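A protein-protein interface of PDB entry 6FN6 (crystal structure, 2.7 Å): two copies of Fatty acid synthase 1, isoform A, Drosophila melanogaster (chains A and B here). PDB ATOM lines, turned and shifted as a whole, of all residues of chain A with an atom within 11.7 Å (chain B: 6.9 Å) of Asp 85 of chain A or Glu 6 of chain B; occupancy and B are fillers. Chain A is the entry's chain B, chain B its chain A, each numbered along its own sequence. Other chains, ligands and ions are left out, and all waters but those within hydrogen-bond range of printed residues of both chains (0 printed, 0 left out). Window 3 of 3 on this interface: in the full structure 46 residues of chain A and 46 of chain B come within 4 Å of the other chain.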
ATOM      1  N   GLU A   6     -13.510 -12.526  -7.677  1.00  0.00           N
ATOM      2  CA  GLU A   6     -14.830 -12.271  -8.239  1.00  0.00           C
ATOM      3  C   GLU A   6     -14.863 -12.583  -9.733  1.00  0.00           C
ATOM      4  O   GLU A   6     -13.827 -12.591 -10.399  1.00  0.00           O
ATOM      5  CB  GLU A   6     -15.238 -10.815  -8.001  1.00  0.00           C
ATOM      6  CG  GLU A   6     -14.370  -9.797  -8.736  1.00  0.00           C
ATOM      7  CD  GLU A   6     -14.841  -8.367  -8.539  1.00  0.00           C
ATOM      8  OE1 GLU A   6     -14.163  -7.444  -9.039  1.00  0.00           O
ATOM      9  OE2 GLU A   6     -15.889  -8.165  -7.887  1.00  0.00           O
ATOM     10  N   THR A   7     -16.059 -12.838 -10.253  1.00  0.00           N
ATOM     11  CA  THR A   7     -16.241 -13.101 -11.677  1.00  0.00           C
ATOM     12  C   THR A   7     -16.636 -11.814 -12.399  1.00  0.00           C
ATOM     13  O   THR A   7     -17.567 -11.124 -11.987  1.00  0.00           O
ATOM     14  CB  THR A   7     -17.312 -14.180 -11.916  1.00  0.00           C
ATOM     15  OG1 THR A   7     -16.970 -15.363 -11.183  1.00  0.00           O
ATOM     16  CG2 THR A   7     -17.418 -14.520 -13.401  1.00  0.00           C
ATOM     17  N   THR A  44     -24.110 -16.986 -14.021  1.00  0.00           N
ATOM     18  CA  THR A  44     -22.774 -17.268 -13.505  1.00  0.00           C
ATOM     19  C   THR A  44     -22.820 -18.333 -12.414  1.00  0.00           C
ATOM     20  O   THR A  44     -21.921 -19.166 -12.317  1.00  0.00           O
ATOM     21  CB  THR A  44     -22.101 -16.006 -12.939  1.00  0.00           C
ATOM     22  OG1 THR A  44     -22.975 -15.373 -11.996  1.00  0.00           O
ATOM     23  CG2 THR A  44     -21.765 -15.034 -14.059  1.00  0.00           C
ATOM     24  N   PHE A  45     -23.872 -18.305 -11.602  1.00  0.00           N
ATOM     25  CA  PHE A  45     -24.017 -19.260 -10.509  1.00  0.00           C
ATOM     26  C   PHE A  45     -24.097 -20.682 -11.050  1.00  0.00           C
ATOM     27  O   PHE A  45     -23.559 -21.610 -10.455  1.00  0.00           O
ATOM     28  CB  PHE A  45     -25.261 -18.944  -9.679  1.00  0.00           C
ATOM     29  CG  PHE A  45     -25.430 -19.830  -8.479  1.00  0.00           C
ATOM     30  CD1 PHE A  45     -24.553 -19.746  -7.410  1.00  0.00           C
ATOM     31  CD2 PHE A  45     -26.467 -20.743  -8.418  1.00  0.00           C
ATOM     32  CE1 PHE A  45     -24.708 -20.559  -6.302  1.00  0.00           C
ATOM     33  CE2 PHE A  45     -26.626 -21.559  -7.311  1.00  0.00           C
ATOM     34  CZ  PHE A  45     -25.746 -21.466  -6.254  1.00  0.00           C
ATOM     35  N   ALA A  46     -24.778 -20.849 -12.177  1.00  0.00           N
ATOM     36  CA  ALA A  46     -24.876 -22.154 -12.819  1.00  0.00           C
ATOM     37  C   ALA A  46     -23.531 -22.538 -13.424  1.00  0.00           C
ATOM     38  O   ALA A  46     -23.174 -23.716 -13.474  1.00  0.00           O
ATOM     39  CB  ALA A  46     -25.960 -22.148 -13.885  1.00  0.00           C
ATOM     40  N   LYS A  47     -22.787 -21.534 -13.876  1.00  0.00           N
ATOM     41  CA  LYS A  47     -21.499 -21.760 -14.521  1.00  0.00           C
ATOM     42  C   LYS A  47     -20.509 -22.412 -13.561  1.00  0.00           C
ATOM     43  O   LYS A  47     -19.856 -23.397 -13.904  1.00  0.00           O
ATOM     44  CB  LYS A  47     -20.929 -20.436 -15.038  1.00  0.00           C
ATOM     45  CG  LYS A  47     -19.805 -20.579 -16.054  1.00  0.00           C
ATOM     46  CD  LYS A  47     -19.400 -19.222 -16.615  1.00  0.00           C
ATOM     47  CE  LYS A  47     -18.184 -19.325 -17.524  1.00  0.00           C
ATOM     48  NZ  LYS A  47     -18.450 -20.117 -18.754  1.00  0.00           N
ATOM     49  N   MET A  48     -20.406 -21.860 -12.358  1.00  0.00           N
ATOM     50  CA  MET A  48     -19.483 -22.384 -11.358  1.00  0.00           C
ATOM     51  C   MET A  48     -20.019 -23.678 -10.744  1.00  0.00           C
ATOM     52  O   MET A  48     -19.246 -24.506 -10.257  1.00  0.00           O
ATOM     53  CB  MET A  48     -19.204 -21.342 -10.263  1.00  0.00           C
ATOM     54  CG  MET A  48     -20.415 -20.564  -9.748  1.00  0.00           C
ATOM     55  SD  MET A  48     -19.975 -19.218  -8.630  1.00  0.00           S
ATOM     56  CE  MET A  48     -19.031 -18.147  -9.719  1.00  0.00           C
ATOM     57  N   GLN A  49     -21.338 -23.848 -10.764  1.00  0.00           N
ATOM     58  CA  GLN A  49     -21.954 -25.088 -10.298  1.00  0.00           C
ATOM     59  C   GLN A  49     -21.792 -26.213 -11.322  1.00  0.00           C
ATOM     60  O   GLN A  49     -22.002 -27.383 -11.004  1.00  0.00           O
ATOM     61  CB  GLN A  49     -23.438 -24.864  -9.998  1.00  0.00           C
ATOM     62  CG  GLN A  49     -23.705 -24.016  -8.762  1.00  0.00           C
ATOM     63  CD  GLN A  49     -23.517 -24.786  -7.469  1.00  0.00           C
ATOM     64  OE1 GLN A  49     -23.580 -26.015  -7.452  1.00  0.00           O
ATOM     65  NE2 GLN A  49     -23.284 -24.064  -6.377  1.00  0.00           N
ATOM     66  N   GLY A  50     -21.414 -25.855 -12.547  1.00  0.00           N
ATOM     67  CA  GLY A  50     -21.128 -26.836 -13.580  1.00  0.00           C
ATOM     68  C   GLY A  50     -22.203 -26.996 -14.643  1.00  0.00           C
ATOM     69  O   GLY A  50     -21.934 -27.522 -15.724  1.00  0.00           O
ATOM     70  N   ILE A  81     -19.151  -9.996 -10.028  1.00  0.00           N
ATOM     71  CA  ILE A  81     -20.037 -10.871  -9.270  1.00  0.00           C
ATOM     72  C   ILE A  81     -19.227 -11.747  -8.316  1.00  0.00           C
ATOM     73  O   ILE A  81     -18.141 -12.216  -8.661  1.00  0.00           O
ATOM     74  CB  ILE A  81     -20.891 -11.736 -10.214  1.00  0.00           C
ATOM     75  CG1 ILE A  81     -21.436 -10.873 -11.363  1.00  0.00           C
ATOM     76  CG2 ILE A  81     -22.011 -12.413  -9.436  1.00  0.00           C
ATOM     77  CD1 ILE A  81     -22.370 -11.596 -12.319  1.00  0.00           C
ATOM     78  N   ASN A  82     -19.758 -11.957  -7.113  1.00  0.00           N
ATOM     79  CA  ASN A  82     -19.095 -12.785  -6.111  1.00  0.00           C
ATOM     80  C   ASN A  82     -20.109 -13.588  -5.299  1.00  0.00           C
ATOM     81  O   ASN A  82     -21.196 -13.100  -4.999  1.00  0.00           O
ATOM     82  CB  ASN A  82     -18.255 -11.914  -5.179  1.00  0.00           C
ATOM     83  CG  ASN A  82     -17.150 -12.689  -4.496  1.00  0.00           C
ATOM     84  OD1 ASN A  82     -17.252 -13.900  -4.303  1.00  0.00           O
ATOM     85  ND2 ASN A  82     -16.086 -11.992  -4.120  1.00  0.00           N
ATOM     86  N   PHE A  83     -19.738 -14.814  -4.933  1.00  0.00           N
ATOM     87  CA  PHE A  83     -20.627 -15.706  -4.187  1.00  0.00           C
ATOM     88  C   PHE A  83     -19.956 -16.284  -2.943  1.00  0.00           C
ATOM     89  O   PHE A  83     -18.768 -16.610  -2.958  1.00  0.00           O
ATOM     90  CB  PHE A  83     -21.106 -16.868  -5.065  1.00  0.00           C
ATOM     91  CG  PHE A  83     -21.999 -16.456  -6.197  1.00  0.00           C
ATOM     92  CD1 PHE A  83     -21.467 -16.083  -7.419  1.00  0.00           C
ATOM     93  CD2 PHE A  83     -23.374 -16.462  -6.045  1.00  0.00           C
ATOM     94  CE1 PHE A  83     -22.288 -15.711  -8.463  1.00  0.00           C
ATOM     95  CE2 PHE A  83     -24.201 -16.092  -7.084  1.00  0.00           C
ATOM     96  CZ  PHE A  83     -23.658 -15.715  -8.296  1.00  0.00           C
ATOM     97  N   PHE A  84     -20.737 -16.407  -1.871  1.00  0.00           N
ATOM     98  CA  PHE A  84     -20.303 -17.097  -0.660  1.00  0.00           C
ATOM     99  C   PHE A  84     -20.800 -18.540  -0.692  1.00  0.00           C
ATOM    100  O   PHE A  84     -22.005 -18.785  -0.696  1.00  0.00           O
ATOM    101  CB  PHE A  84     -20.837 -16.401   0.598  1.00  0.00           C
ATOM    102  CG  PHE A  84     -20.125 -15.118   0.960  1.00  0.00           C
ATOM    103  CD1 PHE A  84     -18.884 -14.801   0.431  1.00  0.00           C
ATOM    104  CD2 PHE A  84     -20.706 -14.235   1.853  1.00  0.00           C
ATOM    105  CE1 PHE A  84     -18.243 -13.624   0.781  1.00  0.00           C
ATOM    106  CE2 PHE A  84     -20.070 -13.061   2.206  1.00  0.00           C
ATOM    107  CZ  PHE A  84     -18.840 -12.755   1.668  1.00  0.00           C
ATOM    108  N   ASP A  85     -19.876 -19.493  -0.706  1.00  0.00           N
ATOM    109  CA  ASP A  85     -20.237 -20.908  -0.685  1.00  0.00           C
ATOM    110  C   ASP A  85     -21.064 -21.251   0.552  1.00  0.00           C
ATOM    111  O   ASP A  85     -21.935 -22.121   0.509  1.00  0.00           O
ATOM    112  CB  ASP A  85     -18.982 -21.780  -0.738  1.00  0.00           C
ATOM    113  CG  ASP A  85     -18.325 -21.770  -2.105  1.00  0.00           C
ATOM    114  OD1 ASP A  85     -18.642 -20.869  -2.911  1.00  0.00           O
ATOM    115  OD2 ASP A  85     -17.487 -22.657  -2.371  1.00  0.00           O
ATOM    116  N   GLY A  86     -20.786 -20.557   1.651  1.00  0.00           N
ATOM    117  CA  GLY A  86     -21.413 -20.848   2.927  1.00  0.00           C
ATOM    118  C   GLY A  86     -22.902 -20.570   2.996  1.00  0.00           C
ATOM    119  O   GLY A  86     -23.684 -21.456   3.336  1.00  0.00           O
ATOM    120  N   THR A  87     -23.294 -19.339   2.683  1.00  0.00           N
ATOM    121  CA  THR A  87     -24.683 -18.911   2.844  1.00  0.00           C
ATOM    122  C   THR A  87     -25.418 -18.786   1.514  1.00  0.00           C
ATOM    123  O   THR A  87     -26.648 -18.816   1.476  1.00  0.00           O
ATOM    124  CB  THR A  87     -24.771 -17.552   3.570  1.00  0.00           C
ATOM    125  OG1 THR A  87     -24.012 -16.572   2.852  1.00  0.00           O
ATOM    126  CG2 THR A  87     -24.243 -17.665   4.988  1.00  0.00           C
ATOM    127  N   GLY A  88     -24.666 -18.636   0.429  1.00  0.00           N
ATOM    128  CA  GLY A  88     -25.259 -18.441  -0.880  1.00  0.00           C
ATOM    129  C   GLY A  88     -25.453 -16.970  -1.191  1.00  0.00           C
ATOM    130  O   GLY A  88     -26.023 -16.609  -2.225  1.00  0.00           O
ATOM    131  N   ALA A  89     -24.987 -16.113  -0.287  1.00  0.00           N
ATOM    132  CA  ALA A  89     -25.077 -14.673  -0.489  1.00  0.00           C
ATOM    133  C   ALA A  89     -24.224 -14.258  -1.676  1.00  0.00           C
ATOM    134  O   ALA A  89     -23.107 -14.750  -1.848  1.00  0.00           O
ATOM    135  CB  ALA A  89     -24.639 -13.931   0.760  1.00  0.00           C
ATOM    136  N   PHE A  90     -24.751 -13.353  -2.495  1.00  0.00           N
ATOM    137  CA  PHE A  90     -24.001 -12.845  -3.633  1.00  0.00           C
ATOM    138  C   PHE A  90     -24.041 -11.326  -3.665  1.00  0.00           C
ATOM    139  O   PHE A  90     -24.854 -10.696  -2.990  1.00  0.00           O
ATOM    140  CB  PHE A  90     -24.552 -13.411  -4.947  1.00  0.00           C
ATOM    141  CG  PHE A  90     -25.847 -12.785  -5.391  1.00  0.00           C
ATOM    142  CD1 PHE A  90     -25.847 -11.665  -6.207  1.00  0.00           C
ATOM    143  CD2 PHE A  90     -27.063 -13.324  -5.005  1.00  0.00           C
ATOM    144  CE1 PHE A  90     -27.033 -11.088  -6.619  1.00  0.00           C
ATOM    145  CE2 PHE A  90     -28.251 -12.751  -5.414  1.00  0.00           C
ATOM    146  CZ  PHE A  90     -28.235 -11.632  -6.224  1.00  0.00           C
ATOM    147  N   GLU A  91     -23.152 -10.747  -4.461  1.00  0.00           N
ATOM    148  CA  GLU A  91     -23.116  -9.309  -4.652  1.00  0.00           C
ATOM    149  C   GLU A  91     -22.667  -9.005  -6.072  1.00  0.00           C
ATOM    150  O   GLU A  91     -21.792  -9.682  -6.612  1.00  0.00           O
ATOM    151  CB  GLU A  91     -22.177  -8.648  -3.644  1.00  0.00           C
ATOM    152  CG  GLU A  91     -22.868  -8.180  -2.379  1.00  0.00           C
ATOM    153  CD  GLU A  91     -21.954  -7.377  -1.476  1.00  0.00           C
ATOM    154  OE1 GLU A  91     -22.326  -7.147  -0.306  1.00  0.00           O
ATOM    155  OE2 GLU A  91     -20.867  -6.969  -1.938  1.00  0.00           O
ATOM    156  N   GLY A 102     -28.026 -10.234  -2.621  1.00  0.00           N
ATOM    157  CA  GLY A 102     -29.060 -11.200  -2.304  1.00  0.00           C
ATOM    158  C   GLY A 102     -28.526 -12.590  -2.016  1.00  0.00           C
ATOM    159  O   GLY A 102     -27.325 -12.783  -1.817  1.00  0.00           O
ATOM    160  N   LYS A 103     -29.433 -13.563  -2.011  1.00  0.00           N
ATOM    161  CA  LYS A 103     -29.087 -14.948  -1.731  1.00  0.00           C
ATOM    162  C   LYS A 103     -29.604 -15.842  -2.850  1.00  0.00           C
ATOM    163  O   LYS A 103     -30.663 -15.581  -3.417  1.00  0.00           O
ATOM    164  CB  LYS A 103     -29.672 -15.376  -0.383  1.00  0.00           C
ATOM    165  CG  LYS A 103     -29.508 -16.851  -0.053  1.00  0.00           C
ATOM    166  CD  LYS A 103     -30.126 -17.183   1.295  1.00  0.00           C
ATOM    167  CE  LYS A 103     -30.113 -18.681   1.564  1.00  0.00           C
ATOM    168  NZ  LYS A 103     -30.677 -19.017   2.902  1.00  0.00           N
ATOM    169  N   ILE A 104     -28.850 -16.891  -3.171  1.00  0.00           N
ATOM    170  CA  ILE A 104     -29.232 -17.812  -4.236  1.00  0.00           C
ATOM    171  C   ILE A 104     -28.898 -19.239  -3.821  1.00  0.00           C
ATOM    172  O   ILE A 104     -27.798 -19.515  -3.344  1.00  0.00           O
ATOM    173  CB  ILE A 104     -28.544 -17.438  -5.562  1.00  0.00           C
ATOM    174  CG1 ILE A 104     -29.119 -18.267  -6.711  1.00  0.00           C
ATOM    175  CG2 ILE A 104     -27.035 -17.647  -5.465  1.00  0.00           C
ATOM    176  CD1 ILE A 104     -28.724 -17.762  -8.090  1.00  0.00           C
ATOM    177  N   THR A 105     -29.857 -20.144  -3.990  1.00  0.00           N
ATOM    178  CA  THR A 105     -29.654 -21.541  -3.623  1.00  0.00           C
ATOM    179  C   THR A 105     -30.349 -22.494  -4.591  1.00  0.00           C
ATOM    180  O   THR A 105     -31.397 -22.175  -5.150  1.00  0.00           O
ATOM    181  CB  THR A 105     -30.174 -21.829  -2.202  1.00  0.00           C
ATOM    182  OG1 THR A 105     -31.567 -21.506  -2.125  1.00  0.00           O
ATOM    183  CG2 THR A 105     -29.414 -21.010  -1.172  1.00  0.00           C
ATOM    184  N   ILE A 106     -29.752 -23.665  -4.784  1.00  0.00           N
ATOM    185  CA  ILE A 106     -30.360 -24.720  -5.581  1.00  0.00           C
ATOM    186  C   ILE A 106     -31.235 -25.563  -4.658  1.00  0.00           C
ATOM    187  O   ILE A 106     -30.722 -26.230  -3.765  1.00  0.00           O
ATOM    188  CB  ILE A 106     -29.292 -25.574  -6.293  1.00  0.00           C
ATOM    189  CG1 ILE A 106     -28.553 -24.727  -7.332  1.00  0.00           C
ATOM    190  CG2 ILE A 106     -29.926 -26.801  -6.950  1.00  0.00           C
ATOM    191  CD1 ILE A 106     -27.323 -25.388  -7.921  1.00  0.00           C
ATOM    192  N   GLU B   6     -12.354 -17.964  -4.252  1.00  0.00           N
ATOM    193  CA  GLU B   6     -12.060 -17.880  -2.826  1.00  0.00           C
ATOM    194  C   GLU B   6     -10.616 -18.289  -2.540  1.00  0.00           C
ATOM    195  O   GLU B   6      -9.992 -18.996  -3.333  1.00  0.00           O
ATOM    196  CB  GLU B   6     -13.020 -18.763  -2.026  1.00  0.00           C
ATOM    197  CG  GLU B   6     -12.870 -20.253  -2.293  1.00  0.00           C
ATOM    198  CD  GLU B   6     -13.787 -21.093  -1.424  1.00  0.00           C
ATOM    199  OE1 GLU B   6     -13.810 -22.330  -1.601  1.00  0.00           O
ATOM    200  OE2 GLU B   6     -14.485 -20.517  -0.563  1.00  0.00           O
ATOM    201  N   THR B   7     -10.097 -17.846  -1.401  1.00  0.00           N
ATOM    202  CA  THR B   7      -8.739 -18.190  -0.995  1.00  0.00           C
ATOM    203  C   THR B   7      -8.742 -19.414  -0.084  1.00  0.00           C
ATOM    204  O   THR B   7      -9.462 -19.459   0.912  1.00  0.00           O
ATOM    205  CB  THR B   7      -8.055 -17.015  -0.260  1.00  0.00           C
ATOM    206  OG1 THR B   7      -8.086 -15.843  -1.084  1.00  0.00           O
ATOM    207  CG2 THR B   7      -6.610 -17.355   0.084  1.00  0.00           C
ATOM    208  N   ILE B   8      -7.936 -20.408  -0.443  1.00  0.00           N
ATOM    209  CA  ILE B   8      -7.811 -21.618   0.356  1.00  0.00           C
ATOM    210  C   ILE B   8      -6.580 -21.513   1.246  1.00  0.00           C
ATOM    211  O   ILE B   8      -5.482 -21.230   0.770  1.00  0.00           O
ATOM    212  CB  ILE B   8      -7.734 -22.874  -0.534  1.00  0.00           C
ATOM    213  CG1 ILE B   8      -8.873 -22.883  -1.559  1.00  0.00           C
ATOM    214  CG2 ILE B   8      -7.766 -24.139   0.320  1.00  0.00           C
ATOM    215  CD1 ILE B   8     -10.264 -22.818  -0.953  1.00  0.00           C
ATOM    216  N   PHE B  79      -9.173 -24.253   5.102  1.00  0.00           N
ATOM    217  CA  PHE B  79     -10.068 -23.118   5.313  1.00  0.00           C
ATOM    218  C   PHE B  79     -10.243 -22.325   4.019  1.00  0.00           C
ATOM    219  O   PHE B  79      -9.266 -21.969   3.360  1.00  0.00           O
ATOM    220  CB  PHE B  79      -9.540 -22.195   6.416  1.00  0.00           C
ATOM    221  CG  PHE B  79      -9.468 -22.839   7.774  1.00  0.00           C
ATOM    222  CD1 PHE B  79     -10.622 -23.197   8.453  1.00  0.00           C
ATOM    223  CD2 PHE B  79      -8.245 -23.067   8.382  1.00  0.00           C
ATOM    224  CE1 PHE B  79     -10.555 -23.783   9.708  1.00  0.00           C
ATOM    225  CE2 PHE B  79      -8.172 -23.651   9.634  1.00  0.00           C
ATOM    226  CZ  PHE B  79      -9.330 -24.008  10.297  1.00  0.00           C
ATOM    227  N   GLY B  80     -11.498 -22.061   3.661  1.00  0.00           N
ATOM    228  CA  GLY B  80     -11.826 -21.251   2.499  1.00  0.00           C
ATOM    229  C   GLY B  80     -12.317 -19.868   2.884  1.00  0.00           C
ATOM    230  O   GLY B  80     -13.262 -19.741   3.659  1.00  0.00           O
ATOM    231  N   ILE B  81     -11.674 -18.831   2.350  1.00  0.00           N
ATOM    232  CA  ILE B  81     -12.009 -17.452   2.702  1.00  0.00           C
ATOM    233  C   ILE B  81     -12.473 -16.686   1.465  1.00  0.00           C
ATOM    234  O   ILE B  81     -11.921 -16.856   0.379  1.00  0.00           O
ATOM    235  CB  ILE B  81     -10.813 -16.737   3.359  1.00  0.00           C
ATOM    236  CG1 ILE B  81     -10.149 -17.661   4.386  1.00  0.00           C
ATOM    237  CG2 ILE B  81     -11.274 -15.437   4.006  1.00  0.00           C
ATOM    238  CD1 ILE B  81      -9.005 -17.031   5.163  1.00  0.00           C
ATOM    239  N   ASN B  82     -13.481 -15.832   1.641  1.00  0.00           N
ATOM    240  CA  ASN B  82     -14.024 -15.031   0.543  1.00  0.00           C
ATOM    241  C   ASN B  82     -14.408 -13.629   1.020  1.00  0.00           C
ATOM    242  O   ASN B  82     -14.874 -13.455   2.144  1.00  0.00           O
ATOM    243  CB  ASN B  82     -15.241 -15.724  -0.072  1.00  0.00           C
ATOM    244  CG  ASN B  82     -15.514 -15.272  -1.493  1.00  0.00           C
ATOM    245  OD1 ASN B  82     -15.162 -14.157  -1.882  1.00  0.00           O
ATOM    246  ND2 ASN B  82     -16.147 -16.136  -2.278  1.00  0.00           N
ATOM    247  N   PHE B  83     -14.214 -12.635   0.155  1.00  0.00           N
ATOM    248  CA  PHE B  83     -14.487 -11.241   0.507  1.00  0.00           C
ATOM    249  C   PHE B  83     -15.360 -10.549  -0.541  1.00  0.00           C
ATOM    250  O   PHE B  83     -15.192 -10.767  -1.741  1.00  0.00           O
ATOM    251  CB  PHE B  83     -13.175 -10.467   0.662  1.00  0.00           C
ATOM    252  CG  PHE B  83     -12.321 -10.935   1.803  1.00  0.00           C
ATOM    253  CD1 PHE B  83     -11.416 -11.968   1.625  1.00  0.00           C
ATOM    254  CD2 PHE B  83     -12.407 -10.335   3.046  1.00  0.00           C
ATOM    255  CE1 PHE B  83     -10.621 -12.402   2.668  1.00  0.00           C
ATOM    256  CE2 PHE B  83     -11.614 -10.765   4.095  1.00  0.00           C
ATOM    257  CZ  PHE B  83     -10.721 -11.799   3.904  1.00  0.00           C
ATOM    258  N   GLU B  91     -16.317 -14.407   4.727  1.00  0.00           N
ATOM    259  CA  GLU B  91     -16.744 -15.695   5.261  1.00  0.00           C
ATOM    260  C   GLU B  91     -15.605 -16.706   5.245  1.00  0.00           C
ATOM    261  O   GLU B  91     -14.784 -16.710   4.328  1.00  0.00           O
ATOM    262  CB  GLU B  91     -17.932 -16.243   4.472  1.00  0.00           C
ATOM    263  CG  GLU B  91     -19.274 -15.899   5.080  1.00  0.00           C
ATOM    264  CD  GLU B  91     -20.425 -16.587   4.378  1.00  0.00           C
ATOM    265  OE1 GLU B  91     -21.587 -16.212   4.644  1.00  0.00           O
ATOM    266  OE2 GLU B  91     -20.169 -17.510   3.574  1.00  0.00           O
ATOM    267  N   CYS B  93     -15.019 -20.839   5.429  1.00  0.00           N
ATOM    268  CA  CYS B  93     -15.574 -22.188   5.368  1.00  0.00           C
ATOM    269  C   CYS B  93     -14.463 -23.208   5.596  1.00  0.00           C
ATOM    270  O   CYS B  93     -13.307 -22.952   5.260  1.00  0.00           O
ATOM    271  CB  CYS B  93     -16.269 -22.432   4.028  1.00  0.00           C
ATOM    272  SG  CYS B  93     -17.721 -21.387   3.756  1.00  0.00           S
ATOM    273  N   GLY B  96     -16.960 -27.640   3.858  1.00  0.00           N
ATOM    274  CA  GLY B  96     -18.146 -27.449   3.045  1.00  0.00           C
ATOM    275  C   GLY B  96     -19.285 -26.866   3.859  1.00  0.00           C
ATOM    276  O   GLY B  96     -20.454 -26.995   3.497  1.00  0.00           O
ATOM    277  N   SER B  97     -18.932 -26.226   4.969  1.00  0.00           N
ATOM    278  CA  SER B  97     -19.912 -25.601   5.847  1.00  0.00           C
ATOM    279  C   SER B  97     -19.341 -24.321   6.448  1.00  0.00           C
ATOM    280  O   SER B  97     -18.135 -24.214   6.673  1.00  0.00           O
ATOM    281  CB  SER B  97     -20.340 -26.568   6.954  1.00  0.00           C
ATOM    282  OG  SER B  97     -19.282 -26.816   7.862  1.00  0.00           O
ATOM    283  N   LEU B  98     -20.211 -23.346   6.683  1.00  0.00           N
ATOM    284  CA  LEU B  98     -19.796 -22.051   7.211  1.00  0.00           C
ATOM    285  C   LEU B  98     -19.176 -22.175   8.598  1.00  0.00           C
ATOM    286  O   LEU B  98     -19.707 -22.872   9.462  1.00  0.00           O
ATOM    287  CB  LEU B  98     -20.989 -21.096   7.261  1.00  0.00           C
ATOM    288  CG  LEU B  98     -20.726 -19.726   7.891  1.00  0.00           C
ATOM    289  CD1 LEU B  98     -19.681 -18.954   7.098  1.00  0.00           C
ATOM    290  CD2 LEU B  98     -22.016 -18.935   7.998  1.00  0.00           C
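The backbone carbonyl oxygen of Phe 83 of chain A lies within hydrogen-bond range of the side-chain amide nitrogen of Asn 82 of chain B (2.7 Å).
OD1 of Asn 82 of chain B lies close to OD1 of Asn 82 of chain A (3.2 Å).
The backbone carbonyl oxygen of Phe 83 of chain B is in hydrogen-bond range of the side-chain amide nitrogen of Asn 82 of chain A (2.8 Å).
OG1 of Thr 87 of chain A sits at hydrogen-bond distance from OE1 of Glu 91 of chain B (3.0 Å).
O of Cys 93 of chain B lies within hydrogen-bond range of N of Gly 80 of chain B, at 2.6 Å.
OG1 of Thr 87 of chain A lies close to N of Ala 89 of chain A (3.3 Å).
N of Phe 84 of chain A sits at hydrogen-bond distance from O of Ala 89 of chain A (2.9 Å).
The backbone NH (N) of Glu 91 of chain B sits at hydrogen-bond distance from the backbone carbonyl oxygen (O) of Asn 82 of chain B (3.1 Å).
The backbone carbonyl oxygen of Glu 91 of chain A lies within hydrogen-bond range of the backbone NH of Asn 82 of chain A (3.1 Å).
Among the printed residues, pairs that only touch across the chains: Phe 84 of chain A with Asn 82 of chain B (3.6 Å), Phe 84 of chain A with Glu 91 of chain B (3.2 Å), Asp 85 of chain A with Glu 6 of chain B (3.8 Å), Gly 86 of chain A with Glu 91 of chain B (3.6 Å), Gly 86 of chain A with Cys 93 of chain B (3.8 Å) and Thr 87 of chain A with Leu 98 of chain B (3.95 Å).
Glu 6 of chain A touches none of the printed residues of chain B.
Printed residues of chain B within 4 Å of Phe 83 of chain A: Asn 82 (2.7 Å).
Printed residues of chain B within 4 Å of Gly 86 of chain A: Glu 91 (3.6 Å) and Cys 93 (3.8 Å).
Printed residues of chain B within 4 Å of Thr 87 of chain A: Glu 91 and Leu 98.
Of chain A, only Asp 85 (3.8 Å) comes within 4 Å of Glu 6 of chain B.
Thr 7 of chain B touches none of the printed residues of chain A.
No residue of chain A comes within 4 Å of Ile 8 of chain B.
No residue of chain A comes within 4 Å of Gly 80 of chain B.
Of the printed residues of chain A, Glu 91 of chain B touches Phe 84 (3.2 Å), Gly 86 (3.6 Å) and Thr 87 (3.0 Å).
Cys 93 of chain B touches just one residue of chain A: Gly 86 (3.8 Å).
The nearest residue of chain B that does not touch Asp 85 of chain A is Cys 93 of chain B (4.6 Å).
The nearest residue of chain A that does not touch Glu 6 of chain B is Phe 83 of chain A (6.2 Å).
The nearest printed residue of chain A that does not touch Leu 98 of chain B is Gly 86 of chain A (4.4 Å).
Of the 25 printed residues of chain A, 6 touch a printed residue of chain B.
Printed residues of chain A that touch a printed residue of chain B: Asn 82, Phe 83, Phe 84, Asp 85, Gly 86 and Thr 87.
Hydrophobic or aromatic side chains of chain A within 4 Å of the printed part of chain B: Phe 84.
Along chain B the printed residues that touch a printed residue of chain A span positions 6 to 98.
Asn 82 of chain B touches its own counterpart, Asn 82 of chain A.
Asn 82 of chain A touches Phe 83 of chain B, and with the chains exchanged Phe 83 of chain A touches Asn 82 of chain B.
6 positions are printed for both chains.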
